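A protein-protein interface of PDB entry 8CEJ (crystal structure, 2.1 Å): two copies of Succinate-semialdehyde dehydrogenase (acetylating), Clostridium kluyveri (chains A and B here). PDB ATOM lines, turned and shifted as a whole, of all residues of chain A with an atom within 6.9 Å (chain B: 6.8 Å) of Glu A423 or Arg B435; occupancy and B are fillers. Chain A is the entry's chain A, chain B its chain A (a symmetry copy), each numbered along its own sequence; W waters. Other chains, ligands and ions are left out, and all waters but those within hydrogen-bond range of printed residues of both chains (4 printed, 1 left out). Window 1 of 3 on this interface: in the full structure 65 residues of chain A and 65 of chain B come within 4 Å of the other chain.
The guanidinium group (NH2) of Arg B435 lies within salt-bridge range of the side-chain carboxylate (OE1) of Glu A423 (3.0 Å). O of Arg B435 sits at hydrogen-bond distance from N of Leu A388 (2.8 Å). The backbone NH of Val B433 is in hydrogen-bond range of the side-chain hydroxyl of Ser A422 (3.0 Å). The guanidinium group of Arg B93 sits at hydrogen-bond distance from the backbone carbonyl oxygen of Gly A404 (2.9 Å). O of Leu A388 lies close to O of Ile B436 (2.6 Å). The backbone carbonyl oxygen (O) of Gly A380 is in hydrogen-bond range of the side-chain amino group (NZ) of Lys B100 (2.9 Å). OD1 of Asn A406 is in hydrogen-bond range of NH2 of Arg B93 (2.9 Å). OG of Ser B434 sits at hydrogen-bond distance from O of Ile A385 (2.5 Å). The backbone carbonyl oxygen of Ser A386 is in hydrogen-bond range of the backbone NH of Arg B435 (3.2 Å).
O of Val B98 sits at hydrogen-bond distance from N of Ser B434, at 3.0 Å. The side-chain carboxylate of Glu A423 is in hydrogen-bond range of a ring nitrogen (NE2) of His A429 (2.8 Å). The backbone NH of Ile B436 is in hydrogen-bond range of the backbone carbonyl oxygen of Val B96. The side-chain amide nitrogen of Asn A424 lies within hydrogen-bond range of the backbone carbonyl oxygen of Asn A406, 2.7 Å away. NH1 of Arg A387 is in hydrogen-bond range of O of Gly A412 (2.9 Å). O of Gly A363 is in hydrogen-bond range of OG of Ser A386.
Among the printed residues, pairs that only touch across the chains: Gly A380 with Val B98 (3.8 Å), Ile A385 with Lys B100 (3.9 Å), Ser A386 with Ser B434 (3.3 Å), Arg A387 with Arg B435 (3.5 Å), Leu A388 with Gly B437 (3.8 Å), Gly A404 with Leu B95 (3.5 Å), Phe A405 with Arg B435 (3.7 Å) and Phe A405 with Gly B437 (3.7 Å).
Of the printed residues of chain B, Glu A423 touches Arg B435 (3.0 Å). Arg B435 touches five residues of chain A. Printed residues of chain B within 4 Å of Gly A380: Val B98 (3.8 Å) and Lys B100 (2.9 Å). Printed residues of chain A within 4 Å of Val B98: Gly A380 (3.8 Å). Of the printed residues of chain A, Leu B95 touches Gly A404. Of the printed residues of chain B, Gly A404 touches Arg B93 (2.9 Å) and Leu B95 (3.5 Å). Thr A408 touches none of the printed residues of chain B.
Of the 12 printed residues of chain B, 9 touch a printed residue of chain A. Hydrophobic or aromatic side chains of chain B within 4 Å of the printed part of chain A: Leu B95, Val B98 and Ile B436. Of the 26 printed residues of chain A, 10 touch a printed residue of chain B. Along chain A the printed residues that touch a printed residue of chain B span positions 380 to 423. Among the printed residues, 17 pairs touch across the chains.
No position is printed for both chains.
Water W2 lies within hydrogen-bond range of the backbone carbonyl oxygen (O) of Gly A404 (2.7 Å), the guanidinium group (NE) of Arg B435 (3.1 Å) and the side-chain amide oxygen (OD1) of Asn A406 (3.5 Å). Water W3 lies within hydrogen-bond range of O of Ser A386 (2.8 Å), NH1 of Arg B435 (2.9 Å) and O of Ser A422 (3.1 Å). Water W1 lies within hydrogen-bond range of the side-chain carboxylate (OE1) of Glu A423 (2.9 Å), the backbone carbonyl oxygen (O) of Val B433 (2.9 Å) and the guanidinium group (NH1) of Arg B435 (3.1 Å). Water W4 lies within hydrogen-bond range of OE1 of Glu A423 (3.1 Å), OE1 of Glu A428 (3.2 Å) and NH2 of Arg B435 (3.4 Å).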
ATOM      1  N   GLY A 207     -16.430  37.436  -2.216  1.00  0.00           N
ATOM      2  CA  GLY A 207     -17.051  37.278  -3.509  1.00  0.00           C
ATOM      3  C   GLY A 207     -17.714  35.922  -3.677  1.00  0.00           C
ATOM      4  O   GLY A 207     -17.721  35.080  -2.775  1.00  0.00           O
ATOM      5  N   GLY A 363     -15.089  25.180  -7.569  1.00  0.00           N
ATOM      6  CA  GLY A 363     -15.136  25.760  -6.244  1.00  0.00           C
ATOM      7  C   GLY A 363     -16.517  25.995  -5.678  1.00  0.00           C
ATOM      8  O   GLY A 363     -16.626  26.436  -4.527  1.00  0.00           O
ATOM      9  N   GLY A 380     -16.432  13.848  -2.156  1.00  0.00           N
ATOM     10  CA  GLY A 380     -16.178  15.074  -1.423  1.00  0.00           C
ATOM     11  C   GLY A 380     -14.710  15.376  -1.213  1.00  0.00           C
ATOM     12  O   GLY A 380     -14.354  16.537  -0.987  1.00  0.00           O
ATOM     13  N   ILE A 385     -14.675  21.612  -4.895  1.00  0.00           N
ATOM     14  CA  ILE A 385     -15.952  22.216  -4.537  1.00  0.00           C
ATOM     15  C   ILE A 385     -15.900  22.680  -3.090  1.00  0.00           C
ATOM     16  O   ILE A 385     -15.121  22.177  -2.276  1.00  0.00           O
ATOM     17  CB  ILE A 385     -17.129  21.238  -4.730  1.00  0.00           C
ATOM     18  CG1 ILE A 385     -16.816  19.913  -4.033  1.00  0.00           C
ATOM     19  CG2 ILE A 385     -17.418  21.029  -6.208  1.00  0.00           C
ATOM     20  CD1 ILE A 385     -17.963  18.940  -4.010  1.00  0.00           C
ATOM     21  N   SER A 386     -16.752  23.652  -2.774  1.00  0.00           N
ATOM     22  CA  SER A 386     -16.915  24.105  -1.401  1.00  0.00           C
ATOM     23  C   SER A 386     -18.077  23.428  -0.693  1.00  0.00           C
ATOM     24  O   SER A 386     -18.105  23.408   0.543  1.00  0.00           O
ATOM     25  CB  SER A 386     -17.114  25.623  -1.362  1.00  0.00           C
ATOM     26  OG  SER A 386     -15.993  26.296  -1.907  1.00  0.00           O
ATOM     27  N   ARG A 387     -19.027  22.867  -1.440  1.00  0.00           N
ATOM     28  CA  ARG A 387     -20.220  22.261  -0.865  1.00  0.00           C
ATOM     29  C   ARG A 387     -20.602  21.027  -1.666  1.00  0.00           C
ATOM     30  O   ARG A 387     -20.721  21.094  -2.893  1.00  0.00           O
ATOM     31  CB  ARG A 387     -21.391  23.251  -0.848  1.00  0.00           C
ATOM     32  CG  ARG A 387     -21.229  24.406   0.124  1.00  0.00           C
ATOM     33  CD  ARG A 387     -22.069  25.594  -0.307  1.00  0.00           C
ATOM     34  NE  ARG A 387     -21.635  26.110  -1.600  1.00  0.00           N
ATOM     35  CZ  ARG A 387     -20.703  27.040  -1.758  1.00  0.00           C
ATOM     36  NH1 ARG A 387     -20.103  27.602  -0.722  1.00  0.00           N
ATOM     37  NH2 ARG A 387     -20.363  27.416  -2.988  1.00  0.00           N
ATOM     38  N   LEU A 388     -20.784  19.911  -0.972  1.00  0.00           N
ATOM     39  CA  LEU A 388     -21.362  18.704  -1.547  1.00  0.00           C
ATOM     40  C   LEU A 388     -22.727  18.485  -0.911  1.00  0.00           C
ATOM     41  O   LEU A 388     -22.860  18.556   0.314  1.00  0.00           O
ATOM     42  CB  LEU A 388     -20.458  17.492  -1.318  1.00  0.00           C
ATOM     43  CG  LEU A 388     -20.933  16.169  -1.925  1.00  0.00           C
ATOM     44  CD1 LEU A 388     -21.067  16.283  -3.435  1.00  0.00           C
ATOM     45  CD2 LEU A 388     -19.990  15.036  -1.553  1.00  0.00           C
ATOM     46  N   VAL A 389     -23.738  18.244  -1.740  1.00  0.00           N
ATOM     47  CA  VAL A 389     -25.120  18.117  -1.289  1.00  0.00           C
ATOM     48  C   VAL A 389     -25.570  16.688  -1.563  1.00  0.00           C
ATOM     49  O   VAL A 389     -25.508  16.217  -2.704  1.00  0.00           O
ATOM     50  CB  VAL A 389     -26.031  19.140  -1.984  1.00  0.00           C
ATOM     51  CG1 VAL A 389     -27.392  19.163  -1.334  1.00  0.00           C
ATOM     52  CG2 VAL A 389     -25.399  20.526  -1.939  1.00  0.00           C
ATOM     53  N   GLY A 404     -27.141  21.122   7.222  1.00  0.00           N
ATOM     54  CA  GLY A 404     -26.281  21.901   8.085  1.00  0.00           C
ATOM     55  C   GLY A 404     -25.552  23.054   7.431  1.00  0.00           C
ATOM     56  O   GLY A 404     -24.691  23.662   8.074  1.00  0.00           O
ATOM     57  N   PHE A 405     -25.860  23.376   6.178  1.00  0.00           N
ATOM     58  CA  PHE A 405     -25.224  24.513   5.529  1.00  0.00           C
ATOM     59  C   PHE A 405     -25.740  25.814   6.128  1.00  0.00           C
ATOM     60  O   PHE A 405     -26.935  25.963   6.398  1.00  0.00           O
ATOM     61  CB  PHE A 405     -25.480  24.487   4.022  1.00  0.00           C
ATOM     62  CG  PHE A 405     -24.904  23.285   3.330  1.00  0.00           C
ATOM     63  CD1 PHE A 405     -23.532  23.105   3.254  1.00  0.00           C
ATOM     64  CD2 PHE A 405     -25.732  22.344   2.744  1.00  0.00           C
ATOM     65  CE1 PHE A 405     -22.999  22.002   2.615  1.00  0.00           C
ATOM     66  CE2 PHE A 405     -25.205  21.239   2.102  1.00  0.00           C
ATOM     67  CZ  PHE A 405     -23.837  21.068   2.037  1.00  0.00           C
ATOM     68  N   ASN A 406     -24.832  26.757   6.341  1.00  0.00           N
ATOM     69  CA  ASN A 406     -25.208  28.028   6.947  1.00  0.00           C
ATOM     70  C   ASN A 406     -26.079  28.828   5.985  1.00  0.00           C
ATOM     71  O   ASN A 406     -25.681  29.049   4.835  1.00  0.00           O
ATOM     72  CB  ASN A 406     -23.966  28.827   7.330  1.00  0.00           C
ATOM     73  CG  ASN A 406     -23.232  28.231   8.516  1.00  0.00           C
ATOM     74  OD1 ASN A 406     -23.813  27.500   9.318  1.00  0.00           O
ATOM     75  ND2 ASN A 406     -21.948  28.548   8.638  1.00  0.00           N
ATOM     76  N   THR A 408     -27.641  31.588   3.735  1.00  0.00           N
ATOM     77  CA  THR A 408     -27.026  32.760   3.126  1.00  0.00           C
ATOM     78  C   THR A 408     -27.599  32.951   1.730  1.00  0.00           C
ATOM     79  O   THR A 408     -28.321  32.099   1.207  1.00  0.00           O
ATOM     80  CB  THR A 408     -25.504  32.623   3.044  1.00  0.00           C
ATOM     81  OG1 THR A 408     -24.918  33.913   2.836  1.00  0.00           O
ATOM     82  CG2 THR A 408     -25.126  31.720   1.881  1.00  0.00           C
ATOM     83  N   THR A 410     -24.996  34.480  -0.284  1.00  0.00           N
ATOM     84  CA  THR A 410     -23.659  34.688  -0.837  1.00  0.00           C
ATOM     85  C   THR A 410     -22.851  33.419  -0.593  1.00  0.00           C
ATOM     86  O   THR A 410     -22.365  33.186   0.519  1.00  0.00           O
ATOM     87  CB  THR A 410     -22.993  35.908  -0.202  1.00  0.00           C
ATOM     88  OG1 THR A 410     -23.820  37.062  -0.390  1.00  0.00           O
ATOM     89  CG2 THR A 410     -21.630  36.161  -0.826  1.00  0.00           C
ATOM     90  N   LEU A 411     -22.707  32.595  -1.629  1.00  0.00           N
ATOM     91  CA  LEU A 411     -21.992  31.326  -1.535  1.00  0.00           C
ATOM     92  C   LEU A 411     -20.570  31.519  -2.055  1.00  0.00           C
ATOM     93  O   LEU A 411     -20.360  31.684  -3.261  1.00  0.00           O
ATOM     94  CB  LEU A 411     -22.718  30.229  -2.313  1.00  0.00           C
ATOM     95  CG  LEU A 411     -23.972  29.598  -1.698  1.00  0.00           C
ATOM     96  CD1 LEU A 411     -25.159  30.548  -1.725  1.00  0.00           C
ATOM     97  CD2 LEU A 411     -24.317  28.296  -2.405  1.00  0.00           C
ATOM     98  N   GLY A 412     -19.600  31.491  -1.145  1.00  0.00           N
ATOM     99  CA  GLY A 412     -18.216  31.648  -1.540  1.00  0.00           C
ATOM    100  C   GLY A 412     -17.670  30.399  -2.207  1.00  0.00           C
ATOM    101  O   GLY A 412     -18.018  29.274  -1.858  1.00  0.00           O
ATOM    102  N   CYS A 413     -16.797  30.616  -3.193  1.00  0.00           N
ATOM    103  CA  CYS A 413     -16.223  29.539  -3.989  1.00  0.00           C
ATOM    104  C   CYS A 413     -14.751  29.293  -3.687  1.00  0.00           C
ATOM    105  O   CYS A 413     -14.101  28.524  -4.405  1.00  0.00           O
ATOM    106  CB  CYS A 413     -16.412  29.824  -5.480  1.00  0.00           C
ATOM    107  SG  CYS A 413     -18.113  29.645  -6.046  1.00  0.00           S
ATOM    108  N   GLY A 414     -14.206  29.922  -2.648  1.00  0.00           N
ATOM    109  CA  GLY A 414     -12.828  29.664  -2.281  1.00  0.00           C
ATOM    110  C   GLY A 414     -11.834  30.173  -3.315  1.00  0.00           C
ATOM    111  O   GLY A 414     -12.120  31.060  -4.123  1.00  0.00           O
ATOM    112  N   SER A 420     -12.333  34.696  -1.123  1.00  0.00           N
ATOM    113  CA  SER A 420     -11.556  34.599   0.108  1.00  0.00           C
ATOM    114  C   SER A 420     -11.989  33.424   0.975  1.00  0.00           C
ATOM    115  O   SER A 420     -11.156  32.842   1.677  1.00  0.00           O
ATOM    116  CB  SER A 420     -11.662  35.900   0.904  1.00  0.00           C
ATOM    117  OG  SER A 420     -12.991  36.115   1.344  1.00  0.00           O
ATOM    118  N   ILE A 421     -13.269  33.063   0.946  1.00  0.00           N
ATOM    119  CA  ILE A 421     -13.786  31.973   1.763  1.00  0.00           C
ATOM    120  C   ILE A 421     -14.386  30.909   0.856  1.00  0.00           C
ATOM    121  O   ILE A 421     -14.955  31.208  -0.199  1.00  0.00           O
ATOM    122  CB  ILE A 421     -14.828  32.465   2.792  1.00  0.00           C
ATOM    123  CG1 ILE A 421     -16.045  33.067   2.085  1.00  0.00           C
ATOM    124  CG2 ILE A 421     -14.206  33.477   3.738  1.00  0.00           C
ATOM    125  CD1 ILE A 421     -17.142  33.504   3.031  1.00  0.00           C
ATOM    126  N   SER A 422     -14.248  29.656   1.274  1.00  0.00           N
ATOM    127  CA  SER A 422     -14.833  28.514   0.571  1.00  0.00           C
ATOM    128  C   SER A 422     -16.064  28.003   1.305  1.00  0.00           C
ATOM    129  O   SER A 422     -16.239  26.804   1.518  1.00  0.00           O
ATOM    130  CB  SER A 422     -13.798  27.409   0.408  1.00  0.00           C
ATOM    131  OG  SER A 422     -13.424  26.876   1.666  1.00  0.00           O
ATOM    132  N   GLU A 423     -16.931  28.927   1.705  1.00  0.00           N
ATOM    133  CA  GLU A 423     -18.086  28.596   2.527  1.00  0.00           C
ATOM    134  C   GLU A 423     -19.156  29.656   2.313  1.00  0.00           C
ATOM    135  O   GLU A 423     -18.962  30.632   1.584  1.00  0.00           O
ATOM    136  CB  GLU A 423     -17.695  28.490   4.003  1.00  0.00           C
ATOM    137  CG  GLU A 423     -17.016  29.738   4.540  1.00  0.00           C
ATOM    138  CD  GLU A 423     -16.575  29.594   5.983  1.00  0.00           C
ATOM    139  OE1 GLU A 423     -16.882  28.552   6.599  1.00  0.00           O
ATOM    140  OE2 GLU A 423     -15.920  30.523   6.499  1.00  0.00           O
ATOM    141  N   ASN A 424     -20.296  29.455   2.966  1.00  0.00           N
ATOM    142  CA  ASN A 424     -21.393  30.406   2.900  1.00  0.00           C
ATOM    143  C   ASN A 424     -21.089  31.634   3.750  1.00  0.00           C
ATOM    144  O   ASN A 424     -20.516  31.530   4.837  1.00  0.00           O
ATOM    145  CB  ASN A 424     -22.690  29.745   3.365  1.00  0.00           C
ATOM    146  CG  ASN A 424     -23.217  28.735   2.362  1.00  0.00           C
ATOM    147  OD1 ASN A 424     -22.502  28.324   1.448  1.00  0.00           O
ATOM    148  ND2 ASN A 424     -24.473  28.333   2.527  1.00  0.00           N
ATOM    149  N   LEU A 425     -21.478  32.800   3.244  1.00  0.00           N
ATOM    150  CA  LEU A 425     -21.205  34.057   3.929  1.00  0.00           C
ATOM    151  C   LEU A 425     -22.214  34.269   5.051  1.00  0.00           C
ATOM    152  O   LEU A 425     -23.427  34.255   4.817  1.00  0.00           O
ATOM    153  CB  LEU A 425     -21.253  35.220   2.941  1.00  0.00           C
ATOM    154  CG  LEU A 425     -20.924  36.592   3.532  1.00  0.00           C
ATOM    155  CD1 LEU A 425     -19.421  36.761   3.678  1.00  0.00           C
ATOM    156  CD2 LEU A 425     -21.520  37.714   2.696  1.00  0.00           C
ATOM    157  N   THR A 426     -21.715  34.477   6.267  1.00  0.00           N
ATOM    158  CA  THR A 426     -22.592  34.734   7.402  1.00  0.00           C
ATOM    159  C   THR A 426     -22.129  35.956   8.182  1.00  0.00           C
ATOM    160  O   THR A 426     -21.233  36.685   7.743  1.00  0.00           O
ATOM    161  CB  THR A 426     -22.652  33.520   8.336  1.00  0.00           C
ATOM    162  OG1 THR A 426     -21.338  33.214   8.818  1.00  0.00           O
ATOM    163  CG2 THR A 426     -23.223  32.310   7.617  1.00  0.00           C
ATOM    164  N   GLU A 428     -20.329  35.908  10.643  1.00  0.00           N
ATOM    165  CA  GLU A 428     -18.966  35.687  11.119  1.00  0.00           C
ATOM    166  C   GLU A 428     -17.949  36.455  10.287  1.00  0.00           C
ATOM    167  O   GLU A 428     -16.969  36.986  10.824  1.00  0.00           O
ATOM    168  CB  GLU A 428     -18.636  34.192  11.099  1.00  0.00           C
ATOM    169  CG  GLU A 428     -19.416  33.352  12.096  1.00  0.00           C
ATOM    170  CD  GLU A 428     -18.967  31.902  12.106  1.00  0.00           C
ATOM    171  OE1 GLU A 428     -18.270  31.487  11.156  1.00  0.00           O
ATOM    172  OE2 GLU A 428     -19.307  31.176  13.066  1.00  0.00           O
ATOM    173  N   HIS A 429     -18.159  36.524   8.975  1.00  0.00           N
ATOM    174  CA  HIS A 429     -17.195  37.159   8.089  1.00  0.00           C
ATOM    175  C   HIS A 429     -17.277  38.679   8.109  1.00  0.00           C
ATOM    176  O   HIS A 429     -16.412  39.334   7.518  1.00  0.00           O
ATOM    177  CB  HIS A 429     -17.391  36.649   6.659  1.00  0.00           C
ATOM    178  CG  HIS A 429     -17.487  35.157   6.560  1.00  0.00           C
ATOM    179  ND1 HIS A 429     -18.690  34.487   6.576  1.00  0.00           N
ATOM    180  CD2 HIS A 429     -16.528  34.207   6.456  1.00  0.00           C
ATOM    181  CE1 HIS A 429     -18.470  33.188   6.480  1.00  0.00           C
ATOM    182  NE2 HIS A 429     -17.165  32.991   6.407  1.00  0.00           N
ATOM    183  N   GLU B  90     -19.167  16.388  12.060  1.00  0.00           N
ATOM    184  CA  GLU B  90     -20.128  17.052  12.937  1.00  0.00           C
ATOM    185  C   GLU B  90     -21.493  16.410  12.717  1.00  0.00           C
ATOM    186  O   GLU B  90     -22.329  16.941  11.969  1.00  0.00           O
ATOM    187  CB  GLU B  90     -20.168  18.556  12.674  1.00  0.00           C
ATOM    188  CG  GLU B  90     -20.964  19.344  13.694  1.00  0.00           C
ATOM    189  CD  GLU B  90     -20.809  20.840  13.523  1.00  0.00           C
ATOM    190  OE1 GLU B  90     -20.197  21.266  12.522  1.00  0.00           O
ATOM    191  OE2 GLU B  90     -21.297  21.590  14.395  1.00  0.00           O
ATOM    192  N   ARG B  93     -24.853  18.400  13.076  1.00  0.00           N
ATOM    193  CA  ARG B  93     -25.268  19.216  11.944  1.00  0.00           C
ATOM    194  C   ARG B  93     -25.310  18.434  10.640  1.00  0.00           C
ATOM    195  O   ARG B  93     -25.563  19.030   9.587  1.00  0.00           O
ATOM    196  CB  ARG B  93     -24.340  20.426  11.780  1.00  0.00           C
ATOM    197  CG  ARG B  93     -24.306  21.366  12.971  1.00  0.00           C
ATOM    198  CD  ARG B  93     -23.713  22.711  12.578  1.00  0.00           C
ATOM    199  NE  ARG B  93     -24.634  23.494  11.761  1.00  0.00           N
ATOM    200  CZ  ARG B  93     -24.322  24.633  11.157  1.00  0.00           C
ATOM    201  NH1 ARG B  93     -23.104  25.145  11.235  1.00  0.00           N
ATOM    202  NH2 ARG B  93     -25.254  25.274  10.457  1.00  0.00           N
ATOM    203  N   LEU B  95     -22.800  17.172   9.026  1.00  0.00           N
ATOM    204  CA  LEU B  95     -21.735  17.798   8.257  1.00  0.00           C
ATOM    205  C   LEU B  95     -20.457  16.979   8.351  1.00  0.00           C
ATOM    206  O   LEU B  95     -20.146  16.408   9.401  1.00  0.00           O
ATOM    207  CB  LEU B  95     -21.457  19.222   8.749  1.00  0.00           C
ATOM    208  CG  LEU B  95     -22.398  20.334   8.292  1.00  0.00           C
ATOM    209  CD1 LEU B  95     -21.973  21.657   8.902  1.00  0.00           C
ATOM    210  CD2 LEU B  95     -22.408  20.423   6.780  1.00  0.00           C
ATOM    211  N   VAL B  96     -19.720  16.929   7.244  1.00  0.00           N
ATOM    212  CA  VAL B  96     -18.373  16.375   7.204  1.00  0.00           C
ATOM    213  C   VAL B  96     -17.465  17.423   6.578  1.00  0.00           C
ATOM    214  O   VAL B  96     -17.759  17.933   5.493  1.00  0.00           O
ATOM    215  CB  VAL B  96     -18.310  15.055   6.411  1.00  0.00           C
ATOM    216  CG1 VAL B  96     -16.898  14.499   6.427  1.00  0.00           C
ATOM    217  CG2 VAL B  96     -19.289  14.043   6.979  1.00  0.00           C
ATOM    218  N   TYR B  97     -16.372  17.747   7.262  1.00  0.00           N
ATOM    219  CA  TYR B  97     -15.457  18.795   6.828  1.00  0.00           C
ATOM    220  C   TYR B  97     -14.264  18.181   6.111  1.00  0.00           C
ATOM    221  O   TYR B  97     -13.680  17.202   6.589  1.00  0.00           O
ATOM    222  CB  TYR B  97     -14.989  19.632   8.020  1.00  0.00           C
ATOM    223  CG  TYR B  97     -16.100  20.407   8.693  1.00  0.00           C
ATOM    224  CD1 TYR B  97     -16.914  19.809   9.645  1.00  0.00           C
ATOM    225  CD2 TYR B  97     -16.336  21.738   8.375  1.00  0.00           C
ATOM    226  CE1 TYR B  97     -17.930  20.512  10.260  1.00  0.00           C
ATOM    227  CE2 TYR B  97     -17.350  22.449   8.986  1.00  0.00           C
ATOM    228  CZ  TYR B  97     -18.143  21.832   9.927  1.00  0.00           C
ATOM    229  OH  TYR B  97     -19.154  22.537  10.537  1.00  0.00           O
ATOM    230  N   VAL B  98     -13.906  18.755   4.964  1.00  0.00           N
ATOM    231  CA  VAL B  98     -12.800  18.279   4.141  1.00  0.00           C
ATOM    232  C   VAL B  98     -11.837  19.435   3.920  1.00  0.00           C
ATOM    233  O   VAL B  98     -12.262  20.555   3.611  1.00  0.00           O
ATOM    234  CB  VAL B  98     -13.290  17.713   2.795  1.00  0.00           C
ATOM    235  CG1 VAL B  98     -12.143  17.054   2.046  1.00  0.00           C
ATOM    236  CG2 VAL B  98     -14.431  16.729   3.008  1.00  0.00           C
ATOM    237  N   LYS B 100      -8.878  21.032   1.706  1.00  0.00           N
ATOM    238  CA  LYS B 100      -8.333  20.991   0.361  1.00  0.00           C
ATOM    239  C   LYS B 100      -7.322  22.109   0.171  1.00  0.00           C
ATOM    240  O   LYS B 100      -7.439  23.171   0.792  1.00  0.00           O
ATOM    241  CB  LYS B 100      -9.442  21.122  -0.692  1.00  0.00           C
ATOM    242  CG  LYS B 100     -10.509  20.048  -0.604  1.00  0.00           C
ATOM    243  CD  LYS B 100     -11.515  20.192  -1.728  1.00  0.00           C
ATOM    244  CE  LYS B 100     -12.584  19.122  -1.644  1.00  0.00           C
ATOM    245  NZ  LYS B 100     -13.397  19.247  -0.407  1.00  0.00           N
ATOM    246  N   VAL B 433     -11.885  24.807   3.248  1.00  0.00           N
ATOM    247  CA  VAL B 433     -12.662  23.878   4.057  1.00  0.00           C
ATOM    248  C   VAL B 433     -14.039  23.739   3.425  1.00  0.00           C
ATOM    249  O   VAL B 433     -14.787  24.719   3.325  1.00  0.00           O
ATOM    250  CB  VAL B 433     -12.764  24.347   5.518  1.00  0.00           C
ATOM    251  CG1 VAL B 433     -13.696  23.437   6.300  1.00  0.00           C
ATOM    252  CG2 VAL B 433     -11.386  24.379   6.159  1.00  0.00           C
ATOM    253  N   SER B 434     -14.369  22.527   2.994  1.00  0.00           N
ATOM    254  CA  SER B 434     -15.638  22.226   2.349  1.00  0.00           C
ATOM    255  C   SER B 434     -16.528  21.425   3.290  1.00  0.00           C
ATOM    256  O   SER B 434     -16.116  21.008   4.375  1.00  0.00           O
ATOM    257  CB  SER B 434     -15.412  21.461   1.041  1.00  0.00           C
ATOM    258  OG  SER B 434     -14.531  22.171   0.188  1.00  0.00           O
ATOM    259  N   ARG B 435     -17.769  21.210   2.857  1.00  0.00           N
ATOM    260  CA  ARG B 435     -18.767  20.529   3.669  1.00  0.00           C
ATOM    261  C   ARG B 435     -19.535  19.532   2.815  1.00  0.00           C
ATOM    262  O   ARG B 435     -19.850  19.808   1.654  1.00  0.00           O
ATOM    263  CB  ARG B 435     -19.733  21.533   4.312  1.00  0.00           C
ATOM    264  CG  ARG B 435     -19.088  22.401   5.379  1.00  0.00           C
ATOM    265  CD  ARG B 435     -19.917  23.638   5.677  1.00  0.00           C
ATOM    266  NE  ARG B 435     -19.337  24.431   6.754  1.00  0.00           N
ATOM    267  CZ  ARG B 435     -18.329  25.280   6.601  1.00  0.00           C
ATOM    268  NH1 ARG B 435     -17.755  25.469   5.425  1.00  0.00           N
ATOM    269  NH2 ARG B 435     -17.882  25.953   7.659  1.00  0.00           N
ATOM    270  N   ILE B 436     -19.838  18.373   3.401  1.00  0.00           N
ATOM    271  CA  ILE B 436     -20.539  17.310   2.690  1.00  0.00           C
ATOM    272  C   ILE B 436     -22.041  17.297   2.983  1.00  0.00           C
ATOM    273  O   ILE B 436     -22.805  16.713   2.198  1.00  0.00           O
ATOM    274  CB  ILE B 436     -19.897  15.940   3.009  1.00  0.00           C
ATOM    275  CG1 ILE B 436     -18.397  15.994   2.718  1.00  0.00           C
ATOM    276  CG2 ILE B 436     -20.522  14.820   2.189  1.00  0.00           C
ATOM    277  CD1 ILE B 436     -17.727  14.638   2.668  1.00  0.00           C
ATOM    278  N   GLY B 437     -22.483  17.927   4.073  1.00  0.00           N
ATOM    279  CA  GLY B 437     -23.886  18.210   4.340  1.00  0.00           C
ATOM    280  C   GLY B 437     -24.920  17.179   3.931  1.00  0.00           C
ATOM    281  O   GLY B 437     -25.424  17.207   2.805  1.00  0.00           O
HETATM  282  O   HOH W   1     -14.979  26.922   5.177  1.00  0.00           O
HETATM  283  O   HOH W   2     -22.273  24.864   7.693  1.00  0.00           O
HETATM  284  O   HOH W   3     -18.613  25.135   2.648  1.00  0.00           O
HETATM  285  O   HOH W   4     -18.208  28.914   9.326  1.00  0.00           O
